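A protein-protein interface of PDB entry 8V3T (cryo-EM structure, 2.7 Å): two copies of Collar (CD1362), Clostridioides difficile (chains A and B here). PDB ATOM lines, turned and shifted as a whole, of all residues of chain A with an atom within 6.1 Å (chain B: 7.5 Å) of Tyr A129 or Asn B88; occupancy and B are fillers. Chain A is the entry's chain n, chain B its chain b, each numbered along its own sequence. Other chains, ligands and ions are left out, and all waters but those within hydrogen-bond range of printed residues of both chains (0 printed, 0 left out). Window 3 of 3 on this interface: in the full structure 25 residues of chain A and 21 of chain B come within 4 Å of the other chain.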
ATOM      1  N   MET A   1      13.165 -11.918 -12.399  1.00  0.00           N
ATOM      2  CA  MET A   1      11.978 -12.364 -13.120  1.00  0.00           C
ATOM      3  C   MET A   1      12.031 -11.931 -14.580  1.00  0.00           C
ATOM      4  O   MET A   1      12.002 -10.741 -14.887  1.00  0.00           O
ATOM      5  CB  MET A   1      10.714 -11.823 -12.456  1.00  0.00           C
ATOM      6  CG  MET A   1       9.437 -12.542 -12.857  1.00  0.00           C
ATOM      7  SD  MET A   1       9.229 -14.118 -12.010  1.00  0.00           S
ATOM      8  CE  MET A   1       7.469 -14.101 -11.683  1.00  0.00           C
ATOM      9  N   LYS A   3      10.963 -11.156 -18.370  1.00  0.00           N
ATOM     10  CA  LYS A   3       9.798 -10.499 -18.945  1.00  0.00           C
ATOM     11  C   LYS A   3       9.438 -11.135 -20.283  1.00  0.00           C
ATOM     12  O   LYS A   3      10.318 -11.467 -21.080  1.00  0.00           O
ATOM     13  CB  LYS A   3      10.063  -9.003 -19.132  1.00  0.00           C
ATOM     14  CG  LYS A   3       9.634  -8.134 -17.961  1.00  0.00           C
ATOM     15  CD  LYS A   3      10.704  -8.065 -16.889  1.00  0.00           C
ATOM     16  CE  LYS A   3      10.205  -7.316 -15.663  1.00  0.00           C
ATOM     17  NZ  LYS A   3       9.182  -8.095 -14.912  1.00  0.00           N
ATOM     18  N   ASN A  53       9.944 -20.738  -3.269  1.00  0.00           N
ATOM     19  CA  ASN A  53      10.173 -19.428  -3.869  1.00  0.00           C
ATOM     20  C   ASN A  53      10.427 -19.475  -5.372  1.00  0.00           C
ATOM     21  O   ASN A  53      10.833 -18.458  -5.945  1.00  0.00           O
ATOM     22  CB  ASN A  53      11.345 -18.730  -3.173  1.00  0.00           C
ATOM     23  CG  ASN A  53      10.909 -17.921  -1.971  1.00  0.00           C
ATOM     24  OD1 ASN A  53       9.955 -17.148  -2.041  1.00  0.00           O
ATOM     25  ND2 ASN A  53      11.608 -18.095  -0.855  1.00  0.00           N
ATOM     26  N   ASN A  55       9.145 -21.067  -9.448  1.00  0.00           N
ATOM     27  CA  ASN A  55       8.055 -21.544 -10.283  1.00  0.00           C
ATOM     28  C   ASN A  55       8.618 -22.237 -11.517  1.00  0.00           C
ATOM     29  O   ASN A  55       9.725 -21.929 -11.967  1.00  0.00           O
ATOM     30  CB  ASN A  55       7.151 -20.385 -10.718  1.00  0.00           C
ATOM     31  CG  ASN A  55       5.963 -20.192  -9.802  1.00  0.00           C
ATOM     32  OD1 ASN A  55       5.446 -21.145  -9.228  1.00  0.00           O
ATOM     33  ND2 ASN A  55       5.521 -18.951  -9.663  1.00  0.00           N
ATOM     34  N   SER A 127      12.016 -17.199 -10.214  1.00  0.00           N
ATOM     35  CA  SER A 127      11.848 -16.953  -8.790  1.00  0.00           C
ATOM     36  C   SER A 127      10.760 -15.914  -8.568  1.00  0.00           C
ATOM     37  O   SER A 127      10.635 -14.957  -9.337  1.00  0.00           O
ATOM     38  CB  SER A 127      13.157 -16.478  -8.157  1.00  0.00           C
ATOM     39  OG  SER A 127      13.244 -15.065  -8.175  1.00  0.00           O
ATOM     40  N   VAL A 128       9.980 -16.105  -7.513  1.00  0.00           N
ATOM     41  CA  VAL A 128       8.842 -15.246  -7.234  1.00  0.00           C
ATOM     42  C   VAL A 128       9.276 -14.094  -6.337  1.00  0.00           C
ATOM     43  O   VAL A 128      10.275 -14.171  -5.617  1.00  0.00           O
ATOM     44  CB  VAL A 128       7.689 -16.048  -6.599  1.00  0.00           C
ATOM     45  CG1 VAL A 128       7.403 -17.295  -7.417  1.00  0.00           C
ATOM     46  CG2 VAL A 128       8.021 -16.415  -5.163  1.00  0.00           C
ATOM     47  N   TYR A 129       8.512 -13.006  -6.383  1.00  0.00           N
ATOM     48  CA  TYR A 129       8.812 -11.831  -5.576  1.00  0.00           C
ATOM     49  C   TYR A 129       8.389 -12.044  -4.129  1.00  0.00           C
ATOM     50  O   TYR A 129       7.342 -12.634  -3.850  1.00  0.00           O
ATOM     51  CB  TYR A 129       8.125 -10.579  -6.129  1.00  0.00           C
ATOM     52  CG  TYR A 129       8.263 -10.338  -7.621  1.00  0.00           C
ATOM     53  CD1 TYR A 129       8.964  -9.236  -8.093  1.00  0.00           C
ATOM     54  CD2 TYR A 129       7.655 -11.172  -8.553  1.00  0.00           C
ATOM     55  CE1 TYR A 129       9.091  -8.992  -9.445  1.00  0.00           C
ATOM     56  CE2 TYR A 129       7.777 -10.935  -9.911  1.00  0.00           C
ATOM     57  CZ  TYR A 129       8.496  -9.843 -10.349  1.00  0.00           C
ATOM     58  OH  TYR A 129       8.618  -9.595 -11.696  1.00  0.00           O
ATOM     59  N   GLU A 130       9.214 -11.549  -3.209  1.00  0.00           N
ATOM     60  CA  GLU A 130       8.928 -11.636  -1.786  1.00  0.00           C
ATOM     61  C   GLU A 130       9.643 -10.497  -1.072  1.00  0.00           C
ATOM     62  O   GLU A 130      10.642  -9.964  -1.560  1.00  0.00           O
ATOM     63  CB  GLU A 130       9.354 -12.993  -1.210  1.00  0.00           C
ATOM     64  CG  GLU A 130      10.761 -13.035  -0.611  1.00  0.00           C
ATOM     65  CD  GLU A 130      11.877 -12.784  -1.621  1.00  0.00           C
ATOM     66  OE1 GLU A 130      11.593 -12.559  -2.816  1.00  0.00           O
ATOM     67  OE2 GLU A 130      13.056 -12.810  -1.208  1.00  0.00           O
ATOM     68  N   GLU A 131       9.113 -10.127   0.090  1.00  0.00           N
ATOM     69  CA  GLU A 131       9.688  -9.084   0.928  1.00  0.00           C
ATOM     70  C   GLU A 131      10.146  -9.696   2.243  1.00  0.00           C
ATOM     71  O   GLU A 131       9.371 -10.388   2.913  1.00  0.00           O
ATOM     72  CB  GLU A 131       8.680  -7.957   1.190  1.00  0.00           C
ATOM     73  CG  GLU A 131       8.130  -7.236  -0.047  1.00  0.00           C
ATOM     74  CD  GLU A 131       9.023  -7.342  -1.275  1.00  0.00           C
ATOM     75  OE1 GLU A 131       8.531  -7.799  -2.328  1.00  0.00           O
ATOM     76  OE2 GLU A 131      10.202  -6.932  -1.205  1.00  0.00           O
ATOM     77  N   ASP B  81       2.911  -9.051 -17.779  1.00  0.00           N
ATOM     78  CA  ASP B  81       3.986  -8.967 -16.795  1.00  0.00           C
ATOM     79  C   ASP B  81       3.507  -8.318 -15.502  1.00  0.00           C
ATOM     80  O   ASP B  81       3.816  -8.796 -14.400  1.00  0.00           O
ATOM     81  CB  ASP B  81       5.160  -8.187 -17.381  1.00  0.00           C
ATOM     82  CG  ASP B  81       5.941  -8.989 -18.397  1.00  0.00           C
ATOM     83  OD1 ASP B  81       5.717 -10.213 -18.493  1.00  0.00           O
ATOM     84  OD2 ASP B  81       6.762  -8.391 -19.121  1.00  0.00           O
ATOM     85  N   GLU B  82       2.750  -7.223 -15.615  1.00  0.00           N
ATOM     86  CA  GLU B  82       2.232  -6.585 -14.403  1.00  0.00           C
ATOM     87  C   GLU B  82       1.322  -7.534 -13.623  1.00  0.00           C
ATOM     88  O   GLU B  82       1.442  -7.670 -12.395  1.00  0.00           O
ATOM     89  CB  GLU B  82       1.497  -5.293 -14.753  1.00  0.00           C
ATOM     90  CG  GLU B  82       2.165  -4.478 -15.837  1.00  0.00           C
ATOM     91  CD  GLU B  82       2.267  -3.011 -15.484  1.00  0.00           C
ATOM     92  OE1 GLU B  82       2.418  -2.695 -14.285  1.00  0.00           O
ATOM     93  OE2 GLU B  82       2.197  -2.172 -16.406  1.00  0.00           O
ATOM     94  N   LEU B  83       0.414  -8.216 -14.326  1.00  0.00           N
ATOM     95  CA  LEU B  83      -0.481  -9.160 -13.666  1.00  0.00           C
ATOM     96  C   LEU B  83       0.289 -10.304 -13.029  1.00  0.00           C
ATOM     97  O   LEU B  83      -0.076 -10.775 -11.946  1.00  0.00           O
ATOM     98  CB  LEU B  83      -1.502  -9.704 -14.665  1.00  0.00           C
ATOM     99  CG  LEU B  83      -2.664  -8.782 -15.031  1.00  0.00           C
ATOM    100  CD1 LEU B  83      -3.464  -9.372 -16.177  1.00  0.00           C
ATOM    101  CD2 LEU B  83      -3.551  -8.531 -13.825  1.00  0.00           C
ATOM    102  N   ASN B  84       1.357 -10.763 -13.684  1.00  0.00           N
ATOM    103  CA  ASN B  84       2.202 -11.797 -13.105  1.00  0.00           C
ATOM    104  C   ASN B  84       2.825 -11.321 -11.803  1.00  0.00           C
ATOM    105  O   ASN B  84       2.945 -12.094 -10.844  1.00  0.00           O
ATOM    106  CB  ASN B  84       3.282 -12.205 -14.105  1.00  0.00           C
ATOM    107  CG  ASN B  84       3.654 -13.664 -13.995  1.00  0.00           C
ATOM    108  OD1 ASN B  84       4.826 -14.006 -13.852  1.00  0.00           O
ATOM    109  ND2 ASN B  84       2.657 -14.534 -14.057  1.00  0.00           N
ATOM    110  N   LYS B  85       3.240 -10.052 -11.751  1.00  0.00           N
ATOM    111  CA  LYS B  85       3.748  -9.520 -10.489  1.00  0.00           C
ATOM    112  C   LYS B  85       2.667  -9.498  -9.412  1.00  0.00           C
ATOM    113  O   LYS B  85       2.945  -9.788  -8.243  1.00  0.00           O
ATOM    114  CB  LYS B  85       4.329  -8.116 -10.673  1.00  0.00           C
ATOM    115  CG  LYS B  85       5.743  -8.094 -11.219  1.00  0.00           C
ATOM    116  CD  LYS B  85       6.253  -6.674 -11.429  1.00  0.00           C
ATOM    117  CE  LYS B  85       5.254  -5.799 -12.163  1.00  0.00           C
ATOM    118  NZ  LYS B  85       5.936  -4.671 -12.857  1.00  0.00           N
ATOM    119  N   LEU B  86       1.429  -9.148  -9.781  1.00  0.00           N
ATOM    120  CA  LEU B  86       0.405  -8.906  -8.762  1.00  0.00           C
ATOM    121  C   LEU B  86       0.031 -10.163  -7.977  1.00  0.00           C
ATOM    122  O   LEU B  86      -0.097 -10.113  -6.749  1.00  0.00           O
ATOM    123  CB  LEU B  86      -0.837  -8.286  -9.394  1.00  0.00           C
ATOM    124  CG  LEU B  86      -0.602  -6.885  -9.947  1.00  0.00           C
ATOM    125  CD1 LEU B  86      -1.809  -6.389 -10.715  1.00  0.00           C
ATOM    126  CD2 LEU B  86      -0.268  -5.958  -8.800  1.00  0.00           C
ATOM    127  N   PHE B  87      -0.168 -11.292  -8.653  1.00  0.00           N
ATOM    128  CA  PHE B  87      -0.700 -12.495  -8.017  1.00  0.00           C
ATOM    129  C   PHE B  87       0.382 -13.565  -7.958  1.00  0.00           C
ATOM    130  O   PHE B  87       0.795 -14.090  -8.996  1.00  0.00           O
ATOM    131  CB  PHE B  87      -1.929 -13.007  -8.770  1.00  0.00           C
ATOM    132  CG  PHE B  87      -3.016 -11.980  -8.914  1.00  0.00           C
ATOM    133  CD1 PHE B  87      -3.933 -11.779  -7.897  1.00  0.00           C
ATOM    134  CD2 PHE B  87      -3.116 -11.212 -10.059  1.00  0.00           C
ATOM    135  CE1 PHE B  87      -4.930 -10.833  -8.022  1.00  0.00           C
ATOM    136  CE2 PHE B  87      -4.111 -10.266 -10.189  1.00  0.00           C
ATOM    137  CZ  PHE B  87      -5.019 -10.076  -9.170  1.00  0.00           C
ATOM    138  N   ASN B  88       0.835 -13.892  -6.745  1.00  0.00           N
ATOM    139  CA  ASN B  88       2.003 -14.754  -6.616  1.00  0.00           C
ATOM    140  C   ASN B  88       1.760 -16.089  -5.918  1.00  0.00           C
ATOM    141  O   ASN B  88       1.873 -17.150  -6.540  1.00  0.00           O
ATOM    142  CB  ASN B  88       3.085 -13.984  -5.860  1.00  0.00           C
ATOM    143  CG  ASN B  88       4.469 -14.471  -6.174  1.00  0.00           C
ATOM    144  OD1 ASN B  88       4.715 -15.038  -7.237  1.00  0.00           O
ATOM    145  ND2 ASN B  88       5.392 -14.252  -5.247  1.00  0.00           N
ATOM    146  N   ARG B  89       1.419 -16.051  -4.632  1.00  0.00           N
ATOM    147  CA  ARG B  89       1.195 -17.250  -3.829  1.00  0.00           C
ATOM    148  C   ARG B  89      -0.168 -17.281  -3.160  1.00  0.00           C
ATOM    149  O   ARG B  89      -0.803 -18.337  -3.104  1.00  0.00           O
ATOM    150  CB  ARG B  89       2.287 -17.395  -2.763  1.00  0.00           C
ATOM    151  CG  ARG B  89       3.586 -18.020  -3.257  1.00  0.00           C
ATOM    152  CD  ARG B  89       3.338 -19.444  -3.745  1.00  0.00           C
ATOM    153  NE  ARG B  89       4.568 -20.201  -3.950  1.00  0.00           N
ATOM    154  CZ  ARG B  89       5.154 -20.380  -5.125  1.00  0.00           C
ATOM    155  NH1 ARG B  89       4.632 -19.894  -6.239  1.00  0.00           N
ATOM    156  NH2 ARG B  89       6.284 -21.076  -5.187  1.00  0.00           N
ATOM    157  N   ASN B  90      -0.624 -16.147  -2.639  1.00  0.00           N
ATOM    158  CA  ASN B  90      -1.908 -16.096  -1.960  1.00  0.00           C
ATOM    159  C   ASN B  90      -2.433 -14.672  -2.005  1.00  0.00           C
ATOM    160  O   ASN B  90      -1.683 -13.718  -2.227  1.00  0.00           O
ATOM    161  CB  ASN B  90      -1.800 -16.604  -0.515  1.00  0.00           C
ATOM    162  CG  ASN B  90      -0.719 -15.896   0.283  1.00  0.00           C
ATOM    163  OD1 ASN B  90      -0.591 -14.675   0.240  1.00  0.00           O
ATOM    164  ND2 ASN B  90       0.068 -16.670   1.017  1.00  0.00           N
ATOM    165  N   ILE B  91      -3.739 -14.545  -1.797  1.00  0.00           N
ATOM    166  CA  ILE B  91      -4.395 -13.251  -1.685  1.00  0.00           C
ATOM    167  C   ILE B  91      -5.176 -13.240  -0.381  1.00  0.00           C
ATOM    168  O   ILE B  91      -5.632 -14.282   0.099  1.00  0.00           O
ATOM    169  CB  ILE B  91      -5.319 -12.948  -2.886  1.00  0.00           C
ATOM    170  CG1 ILE B  91      -6.482 -13.935  -2.944  1.00  0.00           C
ATOM    171  CG2 ILE B  91      -4.538 -12.993  -4.186  1.00  0.00           C
ATOM    172  CD1 ILE B  91      -7.439 -13.662  -4.079  1.00  0.00           C
ATOM    173  N   ASN B  99      -4.576 -19.783  -0.820  1.00  0.00           N
ATOM    174  CA  ASN B  99      -3.438 -20.206  -1.628  1.00  0.00           C
ATOM    175  C   ASN B  99      -3.787 -20.214  -3.114  1.00  0.00           C
ATOM    176  O   ASN B  99      -4.915 -20.516  -3.509  1.00  0.00           O
ATOM    177  CB  ASN B  99      -2.966 -21.597  -1.204  1.00  0.00           C
ATOM    178  CG  ASN B  99      -2.411 -21.625   0.205  1.00  0.00           C
ATOM    179  OD1 ASN B  99      -1.635 -20.754   0.597  1.00  0.00           O
ATOM    180  ND2 ASN B  99      -2.820 -22.620   0.979  1.00  0.00           N
ATOM    181  N   ILE B 100      -2.799 -19.878  -3.941  1.00  0.00           N
ATOM    182  CA  ILE B 100      -2.922 -19.939  -5.395  1.00  0.00           C
ATOM    183  C   ILE B 100      -2.146 -21.159  -5.873  1.00  0.00           C
ATOM    184  O   ILE B 100      -0.941 -21.272  -5.624  1.00  0.00           O
ATOM    185  CB  ILE B 100      -2.397 -18.657  -6.061  1.00  0.00           C
ATOM    186  CG1 ILE B 100      -3.232 -17.453  -5.628  1.00  0.00           C
ATOM    187  CG2 ILE B 100      -2.410 -18.797  -7.579  1.00  0.00           C
ATOM    188  CD1 ILE B 100      -2.723 -16.136  -6.148  1.00  0.00           C
ATOM    189  N   THR B 101      -2.830 -22.071  -6.562  1.00  0.00           N
ATOM    190  CA  THR B 101      -2.249 -23.359  -6.921  1.00  0.00           C
ATOM    191  C   THR B 101      -1.588 -23.368  -8.293  1.00  0.00           C
ATOM    192  O   THR B 101      -0.556 -24.020  -8.466  1.00  0.00           O
ATOM    193  CB  THR B 101      -3.318 -24.454  -6.868  1.00  0.00           C
ATOM    194  OG1 THR B 101      -4.517 -23.984  -7.495  1.00  0.00           O
ATOM    195  CG2 THR B 101      -3.618 -24.832  -5.429  1.00  0.00           C
ATOM    196  N   LYS B 102      -2.152 -22.671  -9.276  1.00  0.00           N
ATOM    197  CA  LYS B 102      -1.541 -22.630 -10.595  1.00  0.00           C
ATOM    198  C   LYS B 102      -2.049 -21.415 -11.355  1.00  0.00           C
ATOM    199  O   LYS B 102      -3.071 -20.820 -11.007  1.00  0.00           O
ATOM    200  CB  LYS B 102      -1.814 -23.915 -11.385  1.00  0.00           C
ATOM    201  CG  LYS B 102      -3.257 -24.108 -11.795  1.00  0.00           C
ATOM    202  CD  LYS B 102      -3.399 -25.322 -12.695  1.00  0.00           C
ATOM    203  CE  LYS B 102      -4.857 -25.650 -12.961  1.00  0.00           C
ATOM    204  NZ  LYS B 102      -5.027 -27.038 -13.469  1.00  0.00           N
ATOM    205  N   LEU B 103      -1.312 -21.061 -12.404  1.00  0.00           N
ATOM    206  CA  LEU B 103      -1.613 -19.915 -13.250  1.00  0.00           C
ATOM    207  C   LEU B 103      -1.568 -20.352 -14.705  1.00  0.00           C
ATOM    208  O   LEU B 103      -0.608 -21.002 -15.129  1.00  0.00           O
ATOM    209  CB  LEU B 103      -0.613 -18.778 -13.012  1.00  0.00           C
ATOM    210  CG  LEU B 103      -0.603 -18.100 -11.644  1.00  0.00           C
ATOM    211  CD1 LEU B 103       0.819 -17.863 -11.188  1.00  0.00           C
ATOM    212  CD2 LEU B 103      -1.341 -16.782 -11.720  1.00  0.00           C
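Hydrophobic or aromatic side chains of chain A within 4 Å of the printed part of chain B: Met A1, Val A128 and Tyr A129.
Along chain A the printed residues that touch a printed residue of chain B span positions 1 to 129.
Among the printed residues, no Asp or Glu carboxylate lies within 4 Å of a Lys or Arg side-chain nitrogen of the other chain.
N of Ile B100 sits at hydrogen-bond distance from O of Arg B89 (2.7 Å).
The backbone carbonyl oxygen (O) of Asn A53 lies within hydrogen-bond range of the backbone NH (N) of Val A128, at 3.0 Å.
The side-chain amide nitrogen (ND2) of Asn B88 is in hydrogen-bond range of the backbone carbonyl oxygen (O) of Tyr A129 (2.9 Å).
The guanidinium group (NH1) of Arg B89 is in hydrogen-bond range of the side-chain amide oxygen (OD1) of Asn A55.
Among the printed residues, pairs that only touch across the chains: Met A1 with Asn B84 (3.4 Å), Lys A3 with Asp B81 (3.1 Å), Val A128 with Asn B88 (3.2 Å), Val A128 with Arg B89 (3.98 Å) and Tyr A129 with Lys B85 (3.3 Å).
No position is printed for both chains.
Of the 7 pairs that touch across the chains among the printed residues, none has its exchanged pair printed and touching as well.
Printed residues of chain B within 4 Å of Asn A55: Arg B89 (3.3 Å).
Of the printed residues of chain B, Val A128 touches Asn B88 and Arg B89.
Tyr A129 touches just these residues of chain B: Lys B85 and Asn B88.
Printed residues of chain A within 4 Å of Asp B81: Lys A3.
Printed residues of chain A within 4 Å of Lys B85: Tyr A129.
Leu B86 touches none of the printed residues of chain A.
Of chain A, only Val A128 and Tyr A129 come within 4 Å of Asn B88.
Of the printed residues of chain A, Arg B89 touches Asn A55 (3.3 Å) and Val A128 (3.98 Å).
The nearest residue of chain A that does not touch Asn B88 is Asn A55 (4.7 Å).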
